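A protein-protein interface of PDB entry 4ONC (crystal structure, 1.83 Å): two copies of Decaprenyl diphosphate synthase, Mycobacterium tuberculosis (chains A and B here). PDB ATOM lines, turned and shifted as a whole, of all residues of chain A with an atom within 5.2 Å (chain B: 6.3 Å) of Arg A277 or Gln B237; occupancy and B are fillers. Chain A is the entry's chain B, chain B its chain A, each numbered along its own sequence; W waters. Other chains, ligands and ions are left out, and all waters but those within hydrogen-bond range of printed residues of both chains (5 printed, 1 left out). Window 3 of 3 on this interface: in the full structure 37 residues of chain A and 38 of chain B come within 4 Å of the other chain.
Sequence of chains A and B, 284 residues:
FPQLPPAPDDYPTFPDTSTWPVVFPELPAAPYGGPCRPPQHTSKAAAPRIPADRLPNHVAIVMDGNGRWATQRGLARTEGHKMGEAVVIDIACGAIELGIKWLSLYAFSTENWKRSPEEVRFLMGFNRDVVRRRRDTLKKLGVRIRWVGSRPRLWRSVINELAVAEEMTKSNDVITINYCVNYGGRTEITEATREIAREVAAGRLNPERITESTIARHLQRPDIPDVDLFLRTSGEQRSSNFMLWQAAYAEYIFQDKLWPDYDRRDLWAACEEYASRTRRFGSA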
ATOM      1  N   ARG A  54     -14.382  12.708  28.836  1.00  0.00           N
ATOM      2  CA  ARG A  54     -15.328  12.894  27.698  1.00  0.00           C
ATOM      3  C   ARG A  54     -16.506  11.821  27.786  1.00  0.00           C
ATOM      4  O   ARG A  54     -17.372  11.840  26.940  1.00  0.00           O
ATOM      5  CB  ARG A  54     -14.695  12.716  26.323  1.00  0.00           C
ATOM      6  CG  ARG A  54     -13.460  13.689  26.075  1.00  0.00           C
ATOM      7  CD  ARG A  54     -14.011  15.117  26.114  1.00  0.00           C
ATOM      8  NE  ARG A  54     -14.828  15.445  24.950  1.00  0.00           N
ATOM      9  CZ  ARG A  54     -15.202  16.691  24.656  1.00  0.00           C
ATOM     10  NH1 ARG A  54     -14.785  17.705  25.480  1.00  0.00           N
ATOM     11  NH2 ARG A  54     -15.957  16.955  23.580  1.00  0.00           N
ATOM     12  N   ALA A 250     -29.102  17.546  29.939  1.00  0.00           N
ATOM     13  CA  ALA A 250     -28.508  16.443  29.166  1.00  0.00           C
ATOM     14  C   ALA A 250     -28.391  16.722  27.657  1.00  0.00           C
ATOM     15  O   ALA A 250     -29.189  17.500  27.054  1.00  0.00           O
ATOM     16  CB  ALA A 250     -29.463  15.151  29.337  1.00  0.00           C
ATOM     17  N   GLU A 251     -27.424  16.022  27.055  1.00  0.00           N
ATOM     18  CA  GLU A 251     -27.329  15.820  25.612  1.00  0.00           C
ATOM     19  C   GLU A 251     -28.274  14.723  25.184  1.00  0.00           C
ATOM     20  O   GLU A 251     -28.246  13.688  25.829  1.00  0.00           O
ATOM     21  CB  GLU A 251     -25.878  15.360  25.278  1.00  0.00           C
ATOM     22  CG  GLU A 251     -24.833  16.443  25.657  1.00  0.00           C
ATOM     23  CD  GLU A 251     -24.791  17.584  24.640  1.00  0.00           C
ATOM     24  OE1 GLU A 251     -25.374  17.547  23.491  1.00  0.00           O
ATOM     25  OE2 GLU A 251     -24.182  18.582  25.038  1.00  0.00           O
ATOM     26  N   TYR A 252     -29.047  14.933  24.115  1.00  0.00           N
ATOM     27  CA  TYR A 252     -29.986  13.947  23.555  1.00  0.00           C
ATOM     28  C   TYR A 252     -29.373  13.312  22.299  1.00  0.00           C
ATOM     29  O   TYR A 252     -28.796  14.041  21.452  1.00  0.00           O
ATOM     30  CB  TYR A 252     -31.302  14.574  23.138  1.00  0.00           C
ATOM     31  CG  TYR A 252     -32.161  14.891  24.341  1.00  0.00           C
ATOM     32  CD1 TYR A 252     -32.045  16.099  25.001  1.00  0.00           C
ATOM     33  CD2 TYR A 252     -33.058  13.952  24.850  1.00  0.00           C
ATOM     34  CE1 TYR A 252     -32.827  16.410  26.132  1.00  0.00           C
ATOM     35  CE2 TYR A 252     -33.846  14.266  26.006  1.00  0.00           C
ATOM     36  CZ  TYR A 252     -33.754  15.488  26.612  1.00  0.00           C
ATOM     37  OH  TYR A 252     -34.530  15.783  27.733  1.00  0.00           O
ATOM     38  N   ILE A 253     -29.514  11.976  22.195  1.00  0.00           N
ATOM     39  CA  ILE A 253     -29.252  11.279  20.915  1.00  0.00           C
ATOM     40  C   ILE A 253     -30.456  10.366  20.674  1.00  0.00           C
ATOM     41  O   ILE A 253     -30.802   9.553  21.569  1.00  0.00           O
ATOM     42  CB  ILE A 253     -27.992  10.436  20.972  1.00  0.00           C
ATOM     43  CG1 ILE A 253     -26.789  11.359  21.157  1.00  0.00           C
ATOM     44  CG2 ILE A 253     -27.876   9.611  19.629  1.00  0.00           C
ATOM     45  CD1 ILE A 253     -25.445  10.617  21.272  1.00  0.00           C
ATOM     46  N   PHE A 254     -31.081  10.512  19.513  1.00  0.00           N
ATOM     47  CA  PHE A 254     -32.288   9.780  19.211  1.00  0.00           C
ATOM     48  C   PHE A 254     -31.800   8.730  18.209  1.00  0.00           C
ATOM     49  O   PHE A 254     -31.474   9.081  17.097  1.00  0.00           O
ATOM     50  CB  PHE A 254     -33.247  10.730  18.540  1.00  0.00           C
ATOM     51  CG  PHE A 254     -33.727  11.817  19.483  1.00  0.00           C
ATOM     52  CD1 PHE A 254     -34.096  11.499  20.813  1.00  0.00           C
ATOM     53  CD2 PHE A 254     -33.770  13.114  19.063  1.00  0.00           C
ATOM     54  CE1 PHE A 254     -34.568  12.487  21.684  1.00  0.00           C
ATOM     55  CE2 PHE A 254     -34.245  14.112  19.928  1.00  0.00           C
ATOM     56  CZ  PHE A 254     -34.618  13.785  21.223  1.00  0.00           C
ATOM     57  N   GLU A 273     -20.382   9.494  20.059  1.00  0.00           N
ATOM     58  CA  GLU A 273     -20.958  10.689  19.495  1.00  0.00           C
ATOM     59  C   GLU A 273     -20.983  11.763  20.563  1.00  0.00           C
ATOM     60  O   GLU A 273     -20.519  12.920  20.315  1.00  0.00           O
ATOM     61  CB  GLU A 273     -22.324  10.437  18.945  1.00  0.00           C
ATOM     62  CG  GLU A 273     -23.027  11.725  18.580  1.00  0.00           C
ATOM     63  CD  GLU A 273     -24.388  11.531  17.967  1.00  0.00           C
ATOM     64  OE1 GLU A 273     -24.742  10.378  17.616  1.00  0.00           O
ATOM     65  OE2 GLU A 273     -25.106  12.520  17.826  1.00  0.00           O
ATOM     66  N   TYR A 274     -21.439  11.367  21.754  1.00  0.00           N
ATOM     67  CA  TYR A 274     -21.433  12.285  22.911  1.00  0.00           C
ATOM     68  C   TYR A 274     -20.025  12.801  23.190  1.00  0.00           C
ATOM     69  O   TYR A 274     -19.793  14.008  23.428  1.00  0.00           O
ATOM     70  CB  TYR A 274     -21.986  11.510  24.097  1.00  0.00           C
ATOM     71  CG  TYR A 274     -21.829  12.264  25.397  1.00  0.00           C
ATOM     72  CD1 TYR A 274     -22.846  13.165  25.807  1.00  0.00           C
ATOM     73  CD2 TYR A 274     -20.699  12.088  26.184  1.00  0.00           C
ATOM     74  CE1 TYR A 274     -22.707  13.913  26.999  1.00  0.00           C
ATOM     75  CE2 TYR A 274     -20.555  12.796  27.350  1.00  0.00           C
ATOM     76  CZ  TYR A 274     -21.536  13.710  27.738  1.00  0.00           C
ATOM     77  OH  TYR A 274     -21.338  14.377  28.934  1.00  0.00           O
ATOM     78  N   ALA A 275     -19.026  11.922  23.199  1.00  0.00           N
ATOM     79  CA  ALA A 275     -17.655  12.365  23.515  1.00  0.00           C
ATOM     80  C   ALA A 275     -17.057  13.335  22.512  1.00  0.00           C
ATOM     81  O   ALA A 275     -16.274  14.183  22.881  1.00  0.00           O
ATOM     82  CB  ALA A 275     -16.768  11.117  23.611  1.00  0.00           C
ATOM     83  N   SER A 276     -17.481  13.249  21.252  1.00  0.00           N
ATOM     84  CA  SER A 276     -17.122  14.181  20.235  1.00  0.00           C
ATOM     85  C   SER A 276     -17.803  15.513  20.200  1.00  0.00           C
ATOM     86  O   SER A 276     -17.287  16.385  19.524  1.00  0.00           O
ATOM     87  CB  SER A 276     -17.316  13.557  18.878  1.00  0.00           C
ATOM     88  OG  SER A 276     -16.138  12.794  18.737  1.00  0.00           O
ATOM     89  N   ARG A 277     -18.914  15.681  20.883  1.00  0.00           N
ATOM     90  CA  ARG A 277     -19.649  16.914  20.747  1.00  0.00           C
ATOM     91  C   ARG A 277     -18.828  18.029  21.402  1.00  0.00           C
ATOM     92  O   ARG A 277     -18.244  17.869  22.503  1.00  0.00           O
ATOM     93  CB  ARG A 277     -21.034  16.832  21.412  1.00  0.00           C
ATOM     94  CG  ARG A 277     -22.007  16.064  20.485  1.00  0.00           C
ATOM     95  CD  ARG A 277     -23.410  16.088  21.089  1.00  0.00           C
ATOM     96  NE  ARG A 277     -24.356  15.343  20.258  1.00  0.00           N
ATOM     97  CZ  ARG A 277     -25.635  15.054  20.604  1.00  0.00           C
ATOM     98  NH1 ARG A 277     -26.143  15.453  21.789  1.00  0.00           N
ATOM     99  NH2 ARG A 277     -26.417  14.408  19.730  1.00  0.00           N
ATOM    100  N   THR A 278     -18.738  19.140  20.698  1.00  0.00           N
ATOM    101  CA  THR A 278     -18.049  20.318  21.272  1.00  0.00           C
ATOM    102  C   THR A 278     -18.859  20.800  22.433  1.00  0.00           C
ATOM    103  O   THR A 278     -20.110  20.891  22.342  1.00  0.00           O
ATOM    104  CB  THR A 278     -17.993  21.453  20.247  1.00  0.00           C
ATOM    105  OG1 THR A 278     -17.180  20.966  19.169  1.00  0.00           O
ATOM    106  CG2 THR A 278     -17.327  22.727  20.935  1.00  0.00           C
ATOM    107  N   ARG A 279     -18.169  21.044  23.553  1.00  0.00           N
ATOM    108  CA  ARG A 279     -18.874  21.467  24.732  1.00  0.00           C
ATOM    109  C   ARG A 279     -18.886  22.954  24.715  1.00  0.00           C
ATOM    110  O   ARG A 279     -17.842  23.595  24.766  1.00  0.00           O
ATOM    111  CB  ARG A 279     -18.166  20.927  25.974  1.00  0.00           C
ATOM    112  CG  ARG A 279     -17.979  19.408  25.909  1.00  0.00           C
ATOM    113  CD  ARG A 279     -19.102  18.659  26.627  1.00  0.00           C
ATOM    114  NE  ARG A 279     -18.665  17.298  26.938  1.00  0.00           N
ATOM    115  CZ  ARG A 279     -18.688  16.273  26.098  1.00  0.00           C
ATOM    116  NH1 ARG A 279     -19.174  16.409  24.822  1.00  0.00           N
ATOM    117  NH2 ARG A 279     -18.216  15.114  26.550  1.00  0.00           N
ATOM    118  N   ARG B 232     -34.556  23.771  18.554  1.00  0.00           N
ATOM    119  CA  ARG B 232     -33.312  24.401  18.941  1.00  0.00           C
ATOM    120  C   ARG B 232     -32.492  24.501  17.621  1.00  0.00           C
ATOM    121  O   ARG B 232     -32.495  23.574  16.868  1.00  0.00           O
ATOM    122  CB  ARG B 232     -32.584  23.645  20.009  1.00  0.00           C
ATOM    123  CG  ARG B 232     -31.336  24.448  20.436  1.00  0.00           C
ATOM    124  CD  ARG B 232     -30.990  24.030  21.818  1.00  0.00           C
ATOM    125  NE  ARG B 232     -29.777  24.682  22.219  1.00  0.00           N
ATOM    126  CZ  ARG B 232     -29.377  24.719  23.457  1.00  0.00           C
ATOM    127  NH1 ARG B 232     -30.027  23.914  24.319  1.00  0.00           N
ATOM    128  NH2 ARG B 232     -28.249  25.393  23.780  1.00  0.00           N
ATOM    129  N   GLY B 235     -27.658  23.123  15.685  1.00  0.00           N
ATOM    130  CA  GLY B 235     -27.260  21.687  15.754  1.00  0.00           C
ATOM    131  C   GLY B 235     -27.164  21.207  17.197  1.00  0.00           C
ATOM    132  O   GLY B 235     -26.739  20.067  17.446  1.00  0.00           O
ATOM    133  N   GLU B 236     -27.552  22.032  18.170  1.00  0.00           N
ATOM    134  CA  GLU B 236     -27.263  21.645  19.587  1.00  0.00           C
ATOM    135  C   GLU B 236     -28.461  20.745  19.959  1.00  0.00           C
ATOM    136  O   GLU B 236     -29.579  21.123  19.640  1.00  0.00           O
ATOM    137  CB  GLU B 236     -27.348  22.875  20.549  1.00  0.00           C
ATOM    138  CG  GLU B 236     -26.111  23.772  20.514  1.00  0.00           C
ATOM    139  CD  GLU B 236     -24.794  22.990  20.509  1.00  0.00           C
ATOM    140  OE1 GLU B 236     -24.508  22.244  21.503  1.00  0.00           O
ATOM    141  OE2 GLU B 236     -24.045  23.133  19.477  1.00  0.00           O
ATOM    142  N   GLN B 237     -28.230  19.645  20.679  1.00  0.00           N
ATOM    143  CA  GLN B 237     -29.355  18.705  20.907  1.00  0.00           C
ATOM    144  C   GLN B 237     -29.495  18.573  22.427  1.00  0.00           C
ATOM    145  O   GLN B 237     -29.178  17.528  23.024  1.00  0.00           O
ATOM    146  CB  GLN B 237     -29.023  17.319  20.295  1.00  0.00           C
ATOM    147  CG  GLN B 237     -28.905  17.424  18.763  1.00  0.00           C
ATOM    148  CD  GLN B 237     -29.398  16.142  18.054  1.00  0.00           C
ATOM    149  OE1 GLN B 237     -29.658  16.184  16.887  1.00  0.00           O
ATOM    150  NE2 GLN B 237     -29.610  15.020  18.789  1.00  0.00           N
ATOM    151  N   ARG B 238     -29.943  19.667  23.027  1.00  0.00           N
ATOM    152  CA  ARG B 238     -30.169  19.764  24.507  1.00  0.00           C
ATOM    153  C   ARG B 238     -31.405  20.613  24.698  1.00  0.00           C
ATOM    154  O   ARG B 238     -31.718  21.465  23.820  1.00  0.00           O
ATOM    155  CB  ARG B 238     -29.015  20.546  25.162  1.00  0.00           C
ATOM    156  CG  ARG B 238     -27.766  19.741  25.170  1.00  0.00           C
ATOM    157  CD  ARG B 238     -26.636  20.284  26.033  1.00  0.00           C
ATOM    158  NE  ARG B 238     -26.467  21.722  25.952  1.00  0.00           N
ATOM    159  CZ  ARG B 238     -25.955  22.426  24.928  1.00  0.00           C
ATOM    160  NH1 ARG B 238     -25.563  21.825  23.799  1.00  0.00           N
ATOM    161  NH2 ARG B 238     -25.835  23.765  25.049  1.00  0.00           N
ATOM    162  N   SER B 239     -32.136  20.409  25.790  1.00  0.00           N
ATOM    163  CA  SER B 239     -33.277  21.309  26.022  1.00  0.00           C
ATOM    164  C   SER B 239     -32.772  22.476  26.908  1.00  0.00           C
ATOM    165  O   SER B 239     -33.449  23.488  26.975  1.00  0.00           O
ATOM    166  CB  SER B 239     -34.419  20.594  26.800  1.00  0.00           C
ATOM    167  OG  SER B 239     -34.001  20.287  28.131  1.00  0.00           O
ATOM    168  N   PHE B 254     -34.293  19.174  16.234  1.00  0.00           N
ATOM    169  CA  PHE B 254     -33.079  19.937  16.341  1.00  0.00           C
ATOM    170  C   PHE B 254     -32.594  20.308  14.952  1.00  0.00           C
ATOM    171  O   PHE B 254     -32.386  19.433  14.115  1.00  0.00           O
ATOM    172  CB  PHE B 254     -32.047  19.131  17.098  1.00  0.00           C
ATOM    173  CG  PHE B 254     -32.435  18.859  18.534  1.00  0.00           C
ATOM    174  CD1 PHE B 254     -32.733  19.926  19.386  1.00  0.00           C
ATOM    175  CD2 PHE B 254     -32.366  17.560  19.067  1.00  0.00           C
ATOM    176  CE1 PHE B 254     -33.079  19.722  20.739  1.00  0.00           C
ATOM    177  CE2 PHE B 254     -32.646  17.352  20.435  1.00  0.00           C
ATOM    178  CZ  PHE B 254     -33.015  18.435  21.262  1.00  0.00           C
HETATM  179  O   HOH W   1     -30.009  12.471  17.581  1.00  0.00           O
HETATM  180  O   HOH W   2     -25.779  19.246  21.552  1.00  0.00           O
HETATM  181  O   HOH W   3     -22.141  20.774  20.651  1.00  0.00           O
HETATM  182  O   HOH W   4     -34.150  17.983  29.152  1.00  0.00           O
HETATM  183  O   HOH W   5     -30.880  19.335  28.001  1.00  0.00           O
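Printed residues of chain B that touch a printed residue of chain A: Gln B237, Arg B238 and Phe B254.
Of the 13 printed residues of chain A, 5 touch a printed residue of chain B.
Hydrophobic or aromatic side chains of chain A within 4 Å of the printed part of chain B: Tyr A252 and Phe A254.
Along chain A the printed residues that touch a printed residue of chain B span positions 250 to 277.
Among the printed residues, Asp or Glu carboxylates within 4 Å of a Lys or Arg side-chain nitrogen of the other chain: Glu A251 with Arg B238.
Phe A254 touches its own counterpart, Phe B254.
Position printed for both chains: 254.
Of the 6 pairs that touch across the chains among the printed residues, 1 has its exchanged pair printed and touching as well.
Among the printed residues, merely in contact across the chains: Ala A250 with Arg B238, Glu A251 with Gln B237 and Phe A254 with Phe B254.
Of the printed residues of chain B, Ala A250 touches Arg B238.
Printed residues of chain B within 4 Å of Tyr A252: Gln B237.
Ile A253 touches none of the printed residues of chain B.
Of the printed residues of chain B, Phe A254 touches Phe B254.
Tyr A274 touches none of the printed residues of chain B.
Arg A277 touches one residue of chain B.
Gln B237 touches three residues of chain A.
Of the printed residues of chain A, Arg B238 touches Ala A250 (3.3 Å) and Glu A251 (3.1 Å).
Printed residues of chain A within 4 Å of Phe B254: Phe A254.
NH1 of Arg B232 lies within hydrogen-bond range of O of Arg B238, at 3.0 Å.
The guanidinium group (NH1) of Arg B238 lies within salt-bridge range of the side-chain carboxylate (OE1) of Glu B236, 2.6 Å away.
The guanidinium group (NH2) of Arg A54 is in hydrogen-bond range of the backbone carbonyl oxygen (O) of Arg A277, 2.7 Å away.
The side-chain carboxylate (OE1) of Glu A251 is in salt-bridge range of the guanidinium group (NH1) of Arg A277 (2.8 Å).
The backbone carbonyl oxygen of Tyr A252 sits at hydrogen-bond distance from the guanidinium group of Arg A277 (3.0 Å).
O of Arg A277 is in hydrogen-bond range of NH1 of Arg A279 (2.9 Å).
Water W4 bridges OG of Ser B239 (2.5 Å) and OH of Tyr A252 (2.6 Å).
Water W2 lies within hydrogen-bond range of the side-chain carboxylate (OE1) of Glu A251 (2.6 Å), the backbone NH (N) of Gln B237 (2.6 Å), the side-chain carboxylate (OE1) of Glu B236 (3.3 Å) and the guanidinium group (NH1) of Arg B238 (3.4 Å).
Water W3 bridges O of Thr A278 (2.6 Å) and OE1 of Glu B236 (2.9 Å).
Water W5 lies within hydrogen-bond range of the backbone carbonyl oxygen (O) of Ala A250 (2.7 Å) and the backbone NH (N) of Ser B239 (2.8 Å).
Water W1 lies within hydrogen-bond range of the side-chain amide nitrogen (NE2) of Gln B237 and the backbone NH (N) of Phe A254.
The backbone carbonyl oxygen of Gln B237 is in hydrogen-bond range of the backbone NH of Tyr A252.
The side-chain amide nitrogen (NE2) of Gln B237 sits close to the guanidinium group (NH2) of Arg A277 (3.4 Å).
The side-chain carboxylate of Glu A251 is in salt-bridge range of the guanidinium group of Arg B238.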
